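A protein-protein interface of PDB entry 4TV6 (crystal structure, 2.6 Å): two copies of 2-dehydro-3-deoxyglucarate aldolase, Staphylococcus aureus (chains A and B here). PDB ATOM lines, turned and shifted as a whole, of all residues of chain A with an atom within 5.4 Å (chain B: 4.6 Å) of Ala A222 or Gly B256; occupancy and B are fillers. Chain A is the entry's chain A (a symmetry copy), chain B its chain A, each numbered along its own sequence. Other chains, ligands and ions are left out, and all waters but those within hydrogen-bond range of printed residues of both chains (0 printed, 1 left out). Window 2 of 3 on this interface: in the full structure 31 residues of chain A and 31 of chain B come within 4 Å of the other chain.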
ATOM      1  N   ASP A 218       3.091  -4.433 -21.601  1.00  0.00           N
ATOM      2  CA  ASP A 218       3.272  -4.360 -23.042  1.00  0.00           C
ATOM      3  C   ASP A 218       4.511  -3.563 -23.438  1.00  0.00           C
ATOM      4  O   ASP A 218       4.888  -3.527 -24.604  1.00  0.00           O
ATOM      5  CB  ASP A 218       2.013  -3.756 -23.677  1.00  0.00           C
ATOM      6  CG  ASP A 218       0.969  -4.818 -24.031  1.00  0.00           C
ATOM      7  OD1 ASP A 218       0.990  -5.904 -23.401  1.00  0.00           O
ATOM      8  OD2 ASP A 218       0.102  -4.560 -24.895  1.00  0.00           O
ATOM      9  N   GLU A 219       5.155  -2.958 -22.446  1.00  0.00           N
ATOM     10  CA  GLU A 219       6.363  -2.185 -22.669  1.00  0.00           C
ATOM     11  C   GLU A 219       7.606  -2.990 -22.307  1.00  0.00           C
ATOM     12  O   GLU A 219       8.736  -2.582 -22.601  1.00  0.00           O
ATOM     13  CB  GLU A 219       6.312  -0.891 -21.889  1.00  0.00           C
ATOM     14  CG  GLU A 219       4.970  -0.167 -21.978  1.00  0.00           C
ATOM     15  CD  GLU A 219       4.905   1.092 -21.133  1.00  0.00           C
ATOM     16  OE1 GLU A 219       4.155   1.098 -20.129  1.00  0.00           O
ATOM     17  OE2 GLU A 219       5.579   2.085 -21.494  1.00  0.00           O
ATOM     18  N   ASP A 220       7.387  -4.143 -21.681  1.00  0.00           N
ATOM     19  CA  ASP A 220       8.453  -5.114 -21.476  1.00  0.00           C
ATOM     20  C   ASP A 220       8.778  -5.779 -22.814  1.00  0.00           C
ATOM     21  O   ASP A 220       9.848  -6.364 -22.990  1.00  0.00           O
ATOM     22  CB  ASP A 220       8.053  -6.159 -20.432  1.00  0.00           C
ATOM     23  CG  ASP A 220       7.850  -5.563 -19.055  1.00  0.00           C
ATOM     24  OD1 ASP A 220       8.588  -4.620 -18.707  1.00  0.00           O
ATOM     25  OD2 ASP A 220       6.951  -6.037 -18.326  1.00  0.00           O
ATOM     26  N   ILE A 221       7.843  -5.664 -23.755  1.00  0.00           N
ATOM     27  CA  ILE A 221       8.023  -6.190 -25.104  1.00  0.00           C
ATOM     28  C   ILE A 221       9.121  -5.440 -25.851  1.00  0.00           C
ATOM     29  O   ILE A 221      10.028  -6.051 -26.418  1.00  0.00           O
ATOM     30  CB  ILE A 221       6.716  -6.105 -25.916  1.00  0.00           C
ATOM     31  CG1 ILE A 221       5.644  -7.014 -25.309  1.00  0.00           C
ATOM     32  CG2 ILE A 221       6.963  -6.476 -27.371  1.00  0.00           C
ATOM     33  CD1 ILE A 221       4.320  -6.971 -26.042  1.00  0.00           C
ATOM     34  N   ALA A 222       9.031  -4.114 -25.847  1.00  0.00           N
ATOM     35  CA  ALA A 222       9.999  -3.269 -26.540  1.00  0.00           C
ATOM     36  C   ALA A 222      11.401  -3.452 -25.969  1.00  0.00           C
ATOM     37  O   ALA A 222      12.393  -3.353 -26.690  1.00  0.00           O
ATOM     38  CB  ALA A 222       9.583  -1.808 -26.458  1.00  0.00           C
ATOM     39  N   LYS A 223      11.469  -3.724 -24.671  1.00  0.00           N
ATOM     40  CA  LYS A 223      12.743  -3.928 -23.997  1.00  0.00           C
ATOM     41  C   LYS A 223      13.400  -5.230 -24.440  1.00  0.00           C
ATOM     42  O   LYS A 223      14.608  -5.277 -24.673  1.00  0.00           O
ATOM     43  CB  LYS A 223      12.546  -3.913 -22.479  1.00  0.00           C
ATOM     44  CG  LYS A 223      12.031  -2.584 -21.947  1.00  0.00           C
ATOM     45  CD  LYS A 223      11.600  -2.685 -20.493  1.00  0.00           C
ATOM     46  CE  LYS A 223      10.859  -1.430 -20.057  1.00  0.00           C
ATOM     47  NZ  LYS A 223      10.306  -1.552 -18.680  1.00  0.00           N
ATOM     48  N   TRP A 224      12.603  -6.286 -24.566  1.00  0.00           N
ATOM     49  CA  TRP A 224      13.123  -7.570 -25.017  1.00  0.00           C
ATOM     50  C   TRP A 224      13.507  -7.525 -26.496  1.00  0.00           C
ATOM     51  O   TRP A 224      14.523  -8.090 -26.895  1.00  0.00           O
ATOM     52  CB  TRP A 224      12.104  -8.686 -24.773  1.00  0.00           C
ATOM     53  CG  TRP A 224      12.053  -9.168 -23.352  1.00  0.00           C
ATOM     54  CD1 TRP A 224      10.989  -9.102 -22.501  1.00  0.00           C
ATOM     55  CD2 TRP A 224      13.114  -9.788 -22.620  1.00  0.00           C
ATOM     56  NE1 TRP A 224      11.321  -9.645 -21.283  1.00  0.00           N
ATOM     57  CE2 TRP A 224      12.626 -10.075 -21.328  1.00  0.00           C
ATOM     58  CE3 TRP A 224      14.436 -10.134 -22.923  1.00  0.00           C
ATOM     59  CZ2 TRP A 224      13.402 -10.686 -20.348  1.00  0.00           C
ATOM     60  CZ3 TRP A 224      15.209 -10.739 -21.951  1.00  0.00           C
ATOM     61  CH2 TRP A 224      14.691 -11.009 -20.679  1.00  0.00           C
ATOM     62  N   GLN A 225      12.694  -6.843 -27.298  1.00  0.00           N
ATOM     63  CA  GLN A 225      12.936  -6.742 -28.737  1.00  0.00           C
ATOM     64  C   GLN A 225      14.253  -6.039 -29.052  1.00  0.00           C
ATOM     65  O   GLN A 225      14.935  -6.380 -30.022  1.00  0.00           O
ATOM     66  CB  GLN A 225      11.781  -6.006 -29.421  1.00  0.00           C
ATOM     67  CG  GLN A 225      10.609  -6.900 -29.786  1.00  0.00           C
ATOM     68  CD  GLN A 225       9.424  -6.125 -30.327  1.00  0.00           C
ATOM     69  OE1 GLN A 225       9.334  -4.910 -30.159  1.00  0.00           O
ATOM     70  NE2 GLN A 225       8.504  -6.828 -30.979  1.00  0.00           N
ATOM     71  N   ALA A 226      14.608  -5.058 -28.230  1.00  0.00           N
ATOM     72  CA  ALA A 226      15.851  -4.320 -28.421  1.00  0.00           C
ATOM     73  C   ALA A 226      17.062  -5.202 -28.141  1.00  0.00           C
ATOM     74  O   ALA A 226      18.166  -4.926 -28.609  1.00  0.00           O
ATOM     75  CB  ALA A 226      15.878  -3.094 -27.535  1.00  0.00           C
ATOM     76  N   GLN A 227      16.844  -6.262 -27.372  1.00  0.00           N
ATOM     77  CA  GLN A 227      17.897  -7.214 -27.054  1.00  0.00           C
ATOM     78  C   GLN A 227      17.986  -8.316 -28.107  1.00  0.00           C
ATOM     79  O   GLN A 227      18.917  -9.119 -28.096  1.00  0.00           O
ATOM     80  CB  GLN A 227      17.656  -7.818 -25.667  1.00  0.00           C
ATOM     81  CG  GLN A 227      18.451  -7.159 -24.552  1.00  0.00           C
ATOM     82  CD  GLN A 227      17.825  -7.374 -23.186  1.00  0.00           C
ATOM     83  OE1 GLN A 227      17.051  -8.309 -22.993  1.00  0.00           O
ATOM     84  NE2 GLN A 227      18.158  -6.507 -22.229  1.00  0.00           N
ATOM     85  N   SER B 252      -0.192  -4.139 -28.411  1.00  0.00           N
ATOM     86  CA  SER B 252       1.030  -4.819 -27.983  1.00  0.00           C
ATOM     87  C   SER B 252       2.141  -4.660 -29.016  1.00  0.00           C
ATOM     88  O   SER B 252       3.312  -4.505 -28.663  1.00  0.00           O
ATOM     89  CB  SER B 252       0.765  -6.304 -27.724  1.00  0.00           C
ATOM     90  OG  SER B 252      -0.140  -6.486 -26.651  1.00  0.00           O
ATOM     91  N   LYS B 253       1.775  -4.707 -30.292  1.00  0.00           N
ATOM     92  CA  LYS B 253       2.742  -4.495 -31.363  1.00  0.00           C
ATOM     93  C   LYS B 253       3.058  -3.010 -31.482  1.00  0.00           C
ATOM     94  O   LYS B 253       4.207  -2.621 -31.695  1.00  0.00           O
ATOM     95  CB  LYS B 253       2.207  -5.038 -32.686  1.00  0.00           C
ATOM     96  CG  LYS B 253       1.864  -6.518 -32.656  1.00  0.00           C
ATOM     97  CD  LYS B 253       1.379  -7.001 -34.008  1.00  0.00           C
ATOM     98  CE  LYS B 253       1.088  -8.487 -33.998  1.00  0.00           C
ATOM     99  NZ  LYS B 253       0.653  -8.947 -35.341  1.00  0.00           N
ATOM    100  N   GLN B 254       2.022  -2.190 -31.331  1.00  0.00           N
ATOM    101  CA  GLN B 254       2.153  -0.738 -31.401  1.00  0.00           C
ATOM    102  C   GLN B 254       3.092  -0.197 -30.326  1.00  0.00           C
ATOM    103  O   GLN B 254       3.940   0.652 -30.597  1.00  0.00           O
ATOM    104  CB  GLN B 254       0.780  -0.075 -31.270  1.00  0.00           C
ATOM    105  CG  GLN B 254       0.835   1.434 -31.090  1.00  0.00           C
ATOM    106  CD  GLN B 254      -0.348   1.973 -30.311  1.00  0.00           C
ATOM    107  OE1 GLN B 254      -1.462   2.055 -30.828  1.00  0.00           O
ATOM    108  NE2 GLN B 254      -0.112   2.340 -29.056  1.00  0.00           N
ATOM    109  N   LYS B 255       2.931  -0.695 -29.104  1.00  0.00           N
ATOM    110  CA  LYS B 255       3.766  -0.276 -27.985  1.00  0.00           C
ATOM    111  C   LYS B 255       5.193  -0.790 -28.147  1.00  0.00           C
ATOM    112  O   LYS B 255       6.147  -0.172 -27.669  1.00  0.00           O
ATOM    113  CB  LYS B 255       3.172  -0.771 -26.663  1.00  0.00           C
ATOM    114  CG  LYS B 255       3.987  -0.409 -25.434  1.00  0.00           C
ATOM    115  CD  LYS B 255       4.052   1.095 -25.235  1.00  0.00           C
ATOM    116  CE  LYS B 255       2.710   1.642 -24.783  1.00  0.00           C
ATOM    117  NZ  LYS B 255       2.272   1.027 -23.499  1.00  0.00           N
ATOM    118  N   GLY B 256       5.335  -1.913 -28.843  1.00  0.00           N
ATOM    119  CA  GLY B 256       6.620  -2.571 -29.001  1.00  0.00           C
ATOM    120  C   GLY B 256       7.698  -1.765 -29.704  1.00  0.00           C
ATOM    121  O   GLY B 256       8.861  -2.167 -29.727  1.00  0.00           O
ATOM    122  N   ASP B 257       7.320  -0.628 -30.278  1.00  0.00           N
ATOM    123  CA  ASP B 257       8.274   0.226 -30.976  1.00  0.00           C
ATOM    124  C   ASP B 257       7.936   1.704 -30.805  1.00  0.00           C
ATOM    125  O   ASP B 257       7.716   2.175 -29.689  1.00  0.00           O
ATOM    126  CB  ASP B 257       8.321  -0.137 -32.462  1.00  0.00           C
ATOM    127  CG  ASP B 257       6.947  -0.427 -33.035  1.00  0.00           C
ATOM    128  OD1 ASP B 257       5.944  -0.002 -32.427  1.00  0.00           O
ATOM    129  OD2 ASP B 257       6.870  -1.085 -34.095  1.00  0.00           O
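The backbone carbonyl oxygen (O) of Gly B256 sits close to the side-chain amide oxygen (OE1) of Gln A225 (2.8 Å). The side-chain carboxylate of Asp A218 lies within hydrogen-bond range of the side-chain hydroxyl of Ser B252 (2.6 Å). The side-chain amino group of Lys B255 is in salt-bridge range of the side-chain carboxylate of Glu A219 (3.9 Å).
Among the printed residues, pairs that only touch across the chains: Asp A218 with Lys B255 (3.4 Å), Ala A222 with Gly B256 (3.4 Å), Ile A221 with Ser B252 (3.7 Å) and Ala A222 with Lys B255 (3.99 Å).
Of the printed residues of chain B, Asp A218 touches Ser B252 (2.6 Å) and Lys B255 (3.4 Å). Of the printed residues of chain B, Glu A219 touches Lys B255. Printed residues of chain B within 4 Å of Ala A222: Lys B255 and Gly B256. Trp A224 touches none of the printed residues of chain B. Of the printed residues of chain B, Gln A225 touches Gly B256 (2.8 Å). Printed residues of chain A within 4 Å of Ser B252: Asp A218 (2.6 Å) and Ile A221 (3.7 Å). Of the printed residues of chain A, Lys B255 touches Asp A218 (3.4 Å), Glu A219 (3.3 Å) and Ala A222 (3.99 Å). Asp B257 touches none of the printed residues of chain A. The nearest printed residue of chain B that does not touch Ala A222 is Asp B257 (4.6 Å). The nearest residue of chain A that does not touch Gly B256 is Ile A221 (4.2 Å). The nearest printed residue of chain B that does not touch Ile A221 is Gly B256 (4.2 Å).
Of the 6 printed residues of chain B, 3 touch a printed residue of chain A. Printed residues of chain A that touch a printed residue of chain B: Asp A218, Glu A219, Ile A221, Ala A222 and Gln A225. Hydrophobic or aromatic side chains of chain A that line the printed part of chain B: Ile A221 and Ala A222. Among the printed residues, Asp or Glu carboxylates within 4 Å of a Lys or Arg side-chain nitrogen of the other chain: Glu A219 with Lys B255 (3.9 Å).
No position is printed for both chains.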
